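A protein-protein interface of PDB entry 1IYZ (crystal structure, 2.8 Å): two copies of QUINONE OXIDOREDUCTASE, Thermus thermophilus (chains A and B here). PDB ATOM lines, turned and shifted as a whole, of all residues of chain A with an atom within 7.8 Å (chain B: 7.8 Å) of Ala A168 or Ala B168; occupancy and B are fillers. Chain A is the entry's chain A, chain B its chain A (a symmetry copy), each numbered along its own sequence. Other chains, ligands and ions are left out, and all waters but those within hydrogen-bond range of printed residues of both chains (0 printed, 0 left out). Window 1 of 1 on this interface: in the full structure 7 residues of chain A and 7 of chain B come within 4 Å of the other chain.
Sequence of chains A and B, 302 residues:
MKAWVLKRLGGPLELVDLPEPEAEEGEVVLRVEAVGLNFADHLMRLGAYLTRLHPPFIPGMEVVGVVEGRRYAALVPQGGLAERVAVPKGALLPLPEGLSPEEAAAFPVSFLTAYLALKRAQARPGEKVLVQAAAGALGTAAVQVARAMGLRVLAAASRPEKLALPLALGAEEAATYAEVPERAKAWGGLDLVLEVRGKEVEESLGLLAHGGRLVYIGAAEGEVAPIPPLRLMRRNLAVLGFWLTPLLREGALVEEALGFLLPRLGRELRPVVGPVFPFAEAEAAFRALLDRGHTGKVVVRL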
ATOM      1  N   VAL A 143     -15.243 -22.760  -5.350  1.00  0.00           N
ATOM      2  CA  VAL A 143     -15.877 -22.993  -4.056  1.00  0.00           C
ATOM      3  C   VAL A 143     -16.584 -24.345  -4.028  1.00  0.00           C
ATOM      4  O   VAL A 143     -16.430 -25.114  -3.077  1.00  0.00           O
ATOM      5  CB  VAL A 143     -16.902 -21.895  -3.711  1.00  0.00           C
ATOM      6  CG1 VAL A 143     -17.578 -22.210  -2.375  1.00  0.00           C
ATOM      7  CG2 VAL A 143     -16.207 -20.543  -3.650  1.00  0.00           C
ATOM      8  N   GLN A 144     -17.349 -24.633  -5.076  1.00  0.00           N
ATOM      9  CA  GLN A 144     -18.080 -25.891  -5.153  1.00  0.00           C
ATOM     10  C   GLN A 144     -17.134 -27.089  -5.256  1.00  0.00           C
ATOM     11  O   GLN A 144     -17.239 -28.038  -4.471  1.00  0.00           O
ATOM     12  CB  GLN A 144     -19.038 -25.863  -6.342  1.00  0.00           C
ATOM     13  CG  GLN A 144     -19.989 -24.680  -6.312  1.00  0.00           C
ATOM     14  CD  GLN A 144     -20.921 -24.638  -7.513  1.00  0.00           C
ATOM     15  OE1 GLN A 144     -21.761 -25.525  -7.696  1.00  0.00           O
ATOM     16  NE2 GLN A 144     -20.772 -23.606  -8.344  1.00  0.00           N
ATOM     17  N   LYS A 162     -20.977  -9.009  -2.498  1.00  0.00           N
ATOM     18  CA  LYS A 162     -20.699 -10.181  -3.324  1.00  0.00           C
ATOM     19  C   LYS A 162     -20.471 -11.430  -2.462  1.00  0.00           C
ATOM     20  O   LYS A 162     -20.533 -12.563  -2.953  1.00  0.00           O
ATOM     21  CB  LYS A 162     -19.473  -9.927  -4.216  1.00  0.00           C
ATOM     22  CG  LYS A 162     -19.628  -8.718  -5.139  1.00  0.00           C
ATOM     23  CD  LYS A 162     -18.391  -8.438  -5.993  1.00  0.00           C
ATOM     24  CE  LYS A 162     -18.270  -9.414  -7.150  1.00  0.00           C
ATOM     25  NZ  LYS A 162     -17.212  -8.999  -8.116  1.00  0.00           N
ATOM     26  N   LEU A 163     -20.239 -11.222  -1.172  1.00  0.00           N
ATOM     27  CA  LEU A 163     -19.969 -12.324  -0.258  1.00  0.00           C
ATOM     28  C   LEU A 163     -21.084 -13.333   0.014  1.00  0.00           C
ATOM     29  O   LEU A 163     -20.800 -14.465   0.404  1.00  0.00           O
ATOM     30  CB  LEU A 163     -19.475 -11.764   1.073  1.00  0.00           C
ATOM     31  CG  LEU A 163     -18.266 -10.836   0.969  1.00  0.00           C
ATOM     32  CD1 LEU A 163     -17.845 -10.443   2.355  1.00  0.00           C
ATOM     33  CD2 LEU A 163     -17.120 -11.525   0.243  1.00  0.00           C
ATOM     34  N   ALA A 164     -22.340 -12.948  -0.192  1.00  0.00           N
ATOM     35  CA  ALA A 164     -23.451 -13.862   0.070  1.00  0.00           C
ATOM     36  C   ALA A 164     -23.472 -15.103  -0.815  1.00  0.00           C
ATOM     37  O   ALA A 164     -23.769 -16.196  -0.349  1.00  0.00           O
ATOM     38  CB  ALA A 164     -24.765 -13.127  -0.044  1.00  0.00           C
ATOM     39  N   LEU A 165     -23.169 -14.940  -2.093  1.00  0.00           N
ATOM     40  CA  LEU A 165     -23.167 -16.069  -3.008  1.00  0.00           C
ATOM     41  C   LEU A 165     -22.179 -17.159  -2.560  1.00  0.00           C
ATOM     42  O   LEU A 165     -22.564 -18.316  -2.394  1.00  0.00           O
ATOM     43  CB  LEU A 165     -22.809 -15.600  -4.418  1.00  0.00           C
ATOM     44  CG  LEU A 165     -23.591 -16.197  -5.590  1.00  0.00           C
ATOM     45  CD1 LEU A 165     -22.769 -15.989  -6.875  1.00  0.00           C
ATOM     46  CD2 LEU A 165     -23.865 -17.684  -5.363  1.00  0.00           C
ATOM     47  N   PRO A 166     -20.892 -16.801  -2.355  1.00  0.00           N
ATOM     48  CA  PRO A 166     -19.868 -17.765  -1.929  1.00  0.00           C
ATOM     49  C   PRO A 166     -20.233 -18.476  -0.633  1.00  0.00           C
ATOM     50  O   PRO A 166     -20.040 -19.684  -0.491  1.00  0.00           O
ATOM     51  CB  PRO A 166     -18.625 -16.894  -1.772  1.00  0.00           C
ATOM     52  CG  PRO A 166     -18.849 -15.824  -2.757  1.00  0.00           C
ATOM     53  CD  PRO A 166     -20.281 -15.471  -2.531  1.00  0.00           C
ATOM     54  N   LEU A 167     -20.749 -17.702   0.312  1.00  0.00           N
ATOM     55  CA  LEU A 167     -21.163 -18.217   1.605  1.00  0.00           C
ATOM     56  C   LEU A 167     -22.309 -19.216   1.395  1.00  0.00           C
ATOM     57  O   LEU A 167     -22.430 -20.198   2.119  1.00  0.00           O
ATOM     58  CB  LEU A 167     -21.608 -17.039   2.480  1.00  0.00           C
ATOM     59  CG  LEU A 167     -21.211 -16.935   3.958  1.00  0.00           C
ATOM     60  CD1 LEU A 167     -22.201 -17.704   4.828  1.00  0.00           C
ATOM     61  CD2 LEU A 167     -19.786 -17.445   4.156  1.00  0.00           C
ATOM     62  N   ALA A 168     -23.137 -18.972   0.384  1.00  0.00           N
ATOM     63  CA  ALA A 168     -24.266 -19.843   0.094  1.00  0.00           C
ATOM     64  C   ALA A 168     -23.849 -21.138  -0.587  1.00  0.00           C
ATOM     65  O   ALA A 168     -24.481 -22.172  -0.381  1.00  0.00           O
ATOM     66  CB  ALA A 168     -25.281 -19.108  -0.773  1.00  0.00           C
ATOM     67  N   LEU A 169     -22.795 -21.081  -1.399  1.00  0.00           N
ATOM     68  CA  LEU A 169     -22.299 -22.251  -2.125  1.00  0.00           C
ATOM     69  C   LEU A 169     -21.530 -23.222  -1.235  1.00  0.00           C
ATOM     70  O   LEU A 169     -21.235 -24.346  -1.651  1.00  0.00           O
ATOM     71  CB  LEU A 169     -21.390 -21.818  -3.274  1.00  0.00           C
ATOM     72  CG  LEU A 169     -22.024 -21.123  -4.480  1.00  0.00           C
ATOM     73  CD1 LEU A 169     -20.948 -20.373  -5.277  1.00  0.00           C
ATOM     74  CD2 LEU A 169     -22.745 -22.155  -5.339  1.00  0.00           C
ATOM     75  N   GLY A 170     -21.195 -22.788  -0.021  1.00  0.00           N
ATOM     76  CA  GLY A 170     -20.469 -23.656   0.883  1.00  0.00           C
ATOM     77  C   GLY A 170     -19.285 -23.052   1.617  1.00  0.00           C
ATOM     78  O   GLY A 170     -18.664 -23.718   2.444  1.00  0.00           O
ATOM     79  N   ALA A 171     -18.947 -21.803   1.332  1.00  0.00           N
ATOM     80  CA  ALA A 171     -17.828 -21.189   2.018  1.00  0.00           C
ATOM     81  C   ALA A 171     -18.106 -21.218   3.512  1.00  0.00           C
ATOM     82  O   ALA A 171     -19.209 -20.882   3.940  1.00  0.00           O
ATOM     83  CB  ALA A 171     -17.654 -19.768   1.554  1.00  0.00           C
ATOM     84  N   GLU A 172     -17.110 -21.633   4.296  1.00  0.00           N
ATOM     85  CA  GLU A 172     -17.235 -21.690   5.748  1.00  0.00           C
ATOM     86  C   GLU A 172     -17.289 -20.257   6.281  1.00  0.00           C
ATOM     87  O   GLU A 172     -18.040 -19.940   7.202  1.00  0.00           O
ATOM     88  CB  GLU A 172     -16.049 -22.449   6.343  1.00  0.00           C
ATOM     89  CG  GLU A 172     -16.002 -22.476   7.870  1.00  0.00           C
ATOM     90  CD  GLU A 172     -14.860 -23.324   8.401  1.00  0.00           C
ATOM     91  OE1 GLU A 172     -14.290 -22.971   9.459  1.00  0.00           O
ATOM     92  OE2 GLU A 172     -14.538 -24.349   7.759  1.00  0.00           O
ATOM     93  N   ALA A 174     -16.590 -15.916   4.816  1.00  0.00           N
ATOM     94  CA  ALA A 174     -16.429 -15.054   3.655  1.00  0.00           C
ATOM     95  C   ALA A 174     -15.994 -13.679   4.118  1.00  0.00           C
ATOM     96  O   ALA A 174     -16.464 -13.190   5.143  1.00  0.00           O
ATOM     97  CB  ALA A 174     -17.743 -14.962   2.887  1.00  0.00           C
ATOM     98  N   ARG A 270     -22.879 -26.962  -9.806  1.00  0.00           N
ATOM     99  CA  ARG A 270     -23.796 -26.193 -10.638  1.00  0.00           C
ATOM    100  C   ARG A 270     -23.154 -24.860 -11.006  1.00  0.00           C
ATOM    101  O   ARG A 270     -22.930 -24.006 -10.150  1.00  0.00           O
ATOM    102  CB  ARG A 270     -25.100 -25.926  -9.878  1.00  0.00           C
ATOM    103  CG  ARG A 270     -25.810 -27.157  -9.331  1.00  0.00           C
ATOM    104  CD  ARG A 270     -26.420 -27.983 -10.444  1.00  0.00           C
ATOM    105  NE  ARG A 270     -27.423 -27.255 -11.232  1.00  0.00           N
ATOM    106  CZ  ARG A 270     -28.505 -26.663 -10.724  1.00  0.00           C
ATOM    107  NH1 ARG A 270     -28.739 -26.703  -9.409  1.00  0.00           N
ATOM    108  NH2 ARG A 270     -29.362 -26.041 -11.533  1.00  0.00           N
ATOM    109  N   VAL A 272     -22.593 -21.110 -11.903  1.00  0.00           N
ATOM    110  CA  VAL A 272     -23.346 -19.888 -11.628  1.00  0.00           C
ATOM    111  C   VAL A 272     -23.411 -19.019 -12.886  1.00  0.00           C
ATOM    112  O   VAL A 272     -22.418 -18.440 -13.306  1.00  0.00           O
ATOM    113  CB  VAL A 272     -22.686 -19.063 -10.504  1.00  0.00           C
ATOM    114  CG1 VAL A 272     -23.546 -17.858 -10.175  1.00  0.00           C
ATOM    115  CG2 VAL A 272     -22.463 -19.923  -9.280  1.00  0.00           C
ATOM    116  N   VAL B 143     -35.359 -22.091   2.225  1.00  0.00           N
ATOM    117  CA  VAL B 143     -34.611 -22.973   1.336  1.00  0.00           C
ATOM    118  C   VAL B 143     -33.670 -23.878   2.127  1.00  0.00           C
ATOM    119  O   VAL B 143     -33.620 -25.088   1.893  1.00  0.00           O
ATOM    120  CB  VAL B 143     -33.781 -22.182   0.306  1.00  0.00           C
ATOM    121  CG1 VAL B 143     -32.972 -23.145  -0.567  1.00  0.00           C
ATOM    122  CG2 VAL B 143     -34.703 -21.331  -0.555  1.00  0.00           C
ATOM    123  N   GLN B 144     -32.936 -23.290   3.066  1.00  0.00           N
ATOM    124  CA  GLN B 144     -31.997 -24.054   3.876  1.00  0.00           C
ATOM    125  C   GLN B 144     -32.714 -25.059   4.779  1.00  0.00           C
ATOM    126  O   GLN B 144     -32.388 -26.251   4.771  1.00  0.00           O
ATOM    127  CB  GLN B 144     -31.140 -23.105   4.710  1.00  0.00           C
ATOM    128  CG  GLN B 144     -30.419 -22.063   3.874  1.00  0.00           C
ATOM    129  CD  GLN B 144     -29.590 -21.100   4.709  1.00  0.00           C
ATOM    130  OE1 GLN B 144     -28.618 -21.497   5.358  1.00  0.00           O
ATOM    131  NE2 GLN B 144     -29.978 -19.823   4.703  1.00  0.00           N
ATOM    132  N   LYS B 162     -32.034 -12.540  -9.081  1.00  0.00           N
ATOM    133  CA  LYS B 162     -32.150 -12.945  -7.683  1.00  0.00           C
ATOM    134  C   LYS B 162     -32.090 -14.473  -7.537  1.00  0.00           C
ATOM    135  O   LYS B 162     -31.856 -15.001  -6.444  1.00  0.00           O
ATOM    136  CB  LYS B 162     -33.457 -12.410  -7.078  1.00  0.00           C
ATOM    137  CG  LYS B 162     -33.583 -10.888  -7.145  1.00  0.00           C
ATOM    138  CD  LYS B 162     -34.905 -10.360  -6.584  1.00  0.00           C
ATOM    139  CE  LYS B 162     -34.922 -10.379  -5.067  1.00  0.00           C
ATOM    140  NZ  LYS B 162     -36.099  -9.645  -4.517  1.00  0.00           N
ATOM    141  N   LEU B 163     -32.270 -15.178  -8.648  1.00  0.00           N
ATOM    142  CA  LEU B 163     -32.276 -16.635  -8.633  1.00  0.00           C
ATOM    143  C   LEU B 163     -30.982 -17.363  -8.274  1.00  0.00           C
ATOM    144  O   LEU B 163     -31.030 -18.513  -7.837  1.00  0.00           O
ATOM    145  CB  LEU B 163     -32.774 -17.149  -9.980  1.00  0.00           C
ATOM    146  CG  LEU B 163     -34.136 -16.604 -10.411  1.00  0.00           C
ATOM    147  CD1 LEU B 163     -34.528 -17.266 -11.699  1.00  0.00           C
ATOM    148  CD2 LEU B 163     -35.184 -16.868  -9.339  1.00  0.00           C
ATOM    149  N   ALA B 164     -29.832 -16.716  -8.443  1.00  0.00           N
ATOM    150  CA  ALA B 164     -28.559 -17.367  -8.137  1.00  0.00           C
ATOM    151  C   ALA B 164     -28.372 -17.733  -6.669  1.00  0.00           C
ATOM    152  O   ALA B 164     -27.853 -18.796  -6.353  1.00  0.00           O
ATOM    153  CB  ALA B 164     -27.410 -16.506  -8.602  1.00  0.00           C
ATOM    154  N   LEU B 165     -28.783 -16.854  -5.770  1.00  0.00           N
ATOM    155  CA  LEU B 165     -28.640 -17.121  -4.349  1.00  0.00           C
ATOM    156  C   LEU B 165     -29.384 -18.403  -3.936  1.00  0.00           C
ATOM    157  O   LEU B 165     -28.786 -19.307  -3.353  1.00  0.00           O
ATOM    158  CB  LEU B 165     -29.169 -15.938  -3.537  1.00  0.00           C
ATOM    159  CG  LEU B 165     -28.372 -15.500  -2.307  1.00  0.00           C
ATOM    160  CD1 LEU B 165     -29.300 -14.677  -1.397  1.00  0.00           C
ATOM    161  CD2 LEU B 165     -27.818 -16.711  -1.555  1.00  0.00           C
ATOM    162  N   PRO B 166     -30.698 -18.497  -4.236  1.00  0.00           N
ATOM    163  CA  PRO B 166     -31.500 -19.676  -3.885  1.00  0.00           C
ATOM    164  C   PRO B 166     -30.928 -20.968  -4.454  1.00  0.00           C
ATOM    165  O   PRO B 166     -30.890 -22.000  -3.783  1.00  0.00           O
ATOM    166  CB  PRO B 166     -32.867 -19.347  -4.477  1.00  0.00           C
ATOM    167  CG  PRO B 166     -32.906 -17.877  -4.414  1.00  0.00           C
ATOM    168  CD  PRO B 166     -31.549 -17.497  -4.906  1.00  0.00           C
ATOM    169  N   LEU B 167     -30.501 -20.894  -5.707  1.00  0.00           N
ATOM    170  CA  LEU B 167     -29.916 -22.026  -6.401  1.00  0.00           C
ATOM    171  C   LEU B 167     -28.624 -22.437  -5.680  1.00  0.00           C
ATOM    172  O   LEU B 167     -28.280 -23.611  -5.622  1.00  0.00           O
ATOM    173  CB  LEU B 167     -29.635 -21.618  -7.852  1.00  0.00           C
ATOM    174  CG  LEU B 167     -29.947 -22.550  -9.030  1.00  0.00           C
ATOM    175  CD1 LEU B 167     -28.779 -23.501  -9.276  1.00  0.00           C
ATOM    176  CD2 LEU B 167     -31.240 -23.317  -8.765  1.00  0.00           C
ATOM    177  N   ALA B 168     -27.922 -21.460  -5.113  1.00  0.00           N
ATOM    178  CA  ALA B 168     -26.676 -21.726  -4.410  1.00  0.00           C
ATOM    179  C   ALA B 168     -26.895 -22.342  -3.036  1.00  0.00           C
ATOM    180  O   ALA B 168     -26.075 -23.135  -2.579  1.00  0.00           O
ATOM    181  CB  ALA B 168     -25.870 -20.440  -4.276  1.00  0.00           C
ATOM    182  N   LEU B 169     -27.994 -21.974  -2.378  1.00  0.00           N
ATOM    183  CA  LEU B 169     -28.316 -22.481  -1.043  1.00  0.00           C
ATOM    184  C   LEU B 169     -28.837 -23.914  -1.061  1.00  0.00           C
ATOM    185  O   LEU B 169     -28.950 -24.547  -0.008  1.00  0.00           O
ATOM    186  CB  LEU B 169     -29.362 -21.590  -0.374  1.00  0.00           C
ATOM    187  CG  LEU B 169     -28.945 -20.187   0.070  1.00  0.00           C
ATOM    188  CD1 LEU B 169     -30.188 -19.313   0.278  1.00  0.00           C
ATOM    189  CD2 LEU B 169     -28.107 -20.286   1.340  1.00  0.00           C
ATOM    190  N   GLY B 170     -29.164 -24.419  -2.249  1.00  0.00           N
ATOM    191  CA  GLY B 170     -29.660 -25.777  -2.345  1.00  0.00           C
ATOM    192  C   GLY B 170     -30.883 -26.004  -3.217  1.00  0.00           C
ATOM    193  O   GLY B 170     -31.318 -27.142  -3.389  1.00  0.00           O
ATOM    194  N   ALA B 171     -31.459 -24.947  -3.768  1.00  0.00           N
ATOM    195  CA  ALA B 171     -32.624 -25.123  -4.613  1.00  0.00           C
ATOM    196  C   ALA B 171     -32.247 -26.045  -5.762  1.00  0.00           C
ATOM    197  O   ALA B 171     -31.198 -25.864  -6.377  1.00  0.00           O
ATOM    198  CB  ALA B 171     -33.082 -23.794  -5.147  1.00  0.00           C
ATOM    199  N   GLU B 172     -33.098 -27.034  -6.037  1.00  0.00           N
ATOM    200  CA  GLU B 172     -32.870 -27.976  -7.126  1.00  0.00           C
ATOM    201  C   GLU B 172     -33.042 -27.230  -8.450  1.00  0.00           C
ATOM    202  O   GLU B 172     -32.301 -27.440  -9.409  1.00  0.00           O
ATOM    203  CB  GLU B 172     -33.857 -29.139  -7.024  1.00  0.00           C
ATOM    204  CG  GLU B 172     -33.798 -30.137  -8.178  1.00  0.00           C
ATOM    205  CD  GLU B 172     -34.730 -31.318  -7.974  1.00  0.00           C
ATOM    206  OE1 GLU B 172     -35.284 -31.829  -8.974  1.00  0.00           O
ATOM    207  OE2 GLU B 172     -34.903 -31.738  -6.808  1.00  0.00           O
ATOM    208  N   ALA B 174     -34.609 -23.166 -10.034  1.00  0.00           N
ATOM    209  CA  ALA B 174     -35.000 -21.811  -9.678  1.00  0.00           C
ATOM    210  C   ALA B 174     -35.644 -21.152 -10.879  1.00  0.00           C
ATOM    211  O   ALA B 174     -35.204 -21.350 -12.009  1.00  0.00           O
ATOM    212  CB  ALA B 174     -33.777 -21.016  -9.232  1.00  0.00           C
ATOM    213  N   ARG B 270     -27.398 -21.034   7.822  1.00  0.00           N
ATOM    214  CA  ARG B 270     -26.693 -19.761   7.913  1.00  0.00           C
ATOM    215  C   ARG B 270     -27.588 -18.644   7.392  1.00  0.00           C
ATOM    216  O   ARG B 270     -27.906 -18.586   6.206  1.00  0.00           O
ATOM    217  CB  ARG B 270     -25.412 -19.808   7.073  1.00  0.00           C
ATOM    218  CG  ARG B 270     -24.455 -20.951   7.388  1.00  0.00           C
ATOM    219  CD  ARG B 270     -23.780 -20.754   8.729  1.00  0.00           C
ATOM    220  NE  ARG B 270     -22.981 -19.526   8.807  1.00  0.00           N
ATOM    221  CZ  ARG B 270     -21.992 -19.208   7.969  1.00  0.00           C
ATOM    222  NH1 ARG B 270     -21.669 -20.031   6.967  1.00  0.00           N
ATOM    223  NH2 ARG B 270     -21.318 -18.072   8.140  1.00  0.00           N
ATOM    224  N   VAL B 272     -28.876 -15.359   5.737  1.00  0.00           N
ATOM    225  CA  VAL B 272     -28.340 -14.481   4.699  1.00  0.00           C
ATOM    226  C   VAL B 272     -28.516 -13.016   5.111  1.00  0.00           C
ATOM    227  O   VAL B 272     -29.622 -12.495   5.132  1.00  0.00           O
ATOM    228  CB  VAL B 272     -29.064 -14.694   3.354  1.00  0.00           C
ATOM    229  CG1 VAL B 272     -28.415 -13.843   2.280  1.00  0.00           C
ATOM    230  CG2 VAL B 272     -29.046 -16.157   2.973  1.00  0.00           C
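The backbone carbonyl oxygen of Ala A168 sits close to the backbone carbonyl oxygen of Ala B168 (2.9 Å).
OE1 of Gln A144 is in hydrogen-bond range of N of Arg A270 (2.8 Å). O of Pro A166 is in hydrogen-bond range of N of Ala A171, 3.0 Å away. OE1 of Gln B144 is in hydrogen-bond range of N of Arg B270 (2.8 Å). The backbone NH (N) of Ala B171 is in hydrogen-bond range of the backbone carbonyl oxygen (O) of Pro B166, at 3.0 Å.
Among the printed residues, pairs that only touch across the chains: Leu A165 with Ala B168 (3.6 Å), Leu A167 with Arg B270 (3.2 Å), Ala A168 with Leu B165 (3.6 Å), Ala A168 with Leu B169 (3.7 Å), Leu A169 with Ala B168 (3.7 Å), Ala A171 with Arg B270 (3.99 Å), Glu A172 with Arg B270 (3.6 Å), Arg A270 with Leu B167 (3.2 Å), Arg A270 with Ala B171 (3.99 Å) and Arg A270 with Glu B172 (3.6 Å).
Ala A168 touches three residues of chain B. Printed residues of chain A within 4 Å of Ala B168: Leu A165, Ala A168 and Leu A169. Of the printed residues of chain B, Leu A169 touches Ala B168 (3.7 Å). Printed residues of chain A within 4 Å of Leu B165: Ala A168 (3.6 Å). Of the printed residues of chain B, Leu A165 touches Ala B168. Of the printed residues of chain B, Leu A167 touches Arg B270 (3.2 Å).
Printed residues of chain A that touch a printed residue of chain B: Leu A165, Leu A167, Ala A168, Leu A169, Ala A171, Glu A172 and Arg A270. Hydrophobic or aromatic side chains of chain B within 4 Å of the printed part of chain A: Leu B165, Leu B167, Ala B168 and Leu B169. Among the printed residues, 11 pairs touch across the chains.
Leu A165 touches Ala B168, and with the chains exchanged Ala A168 touches Leu B165. Leu A167 touches Arg B270, and with the chains exchanged Arg A270 touches Leu B167. Ala A171 touches Arg B270, and with the chains exchanged Arg A270 touches Ala B171. Glu A172 touches Arg B270, and with the chains exchanged Arg A270 touches Glu B172. Of the 11 pairs that touch across the chains among the printed residues, 11 have their exchanged pair printed and touching as well.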
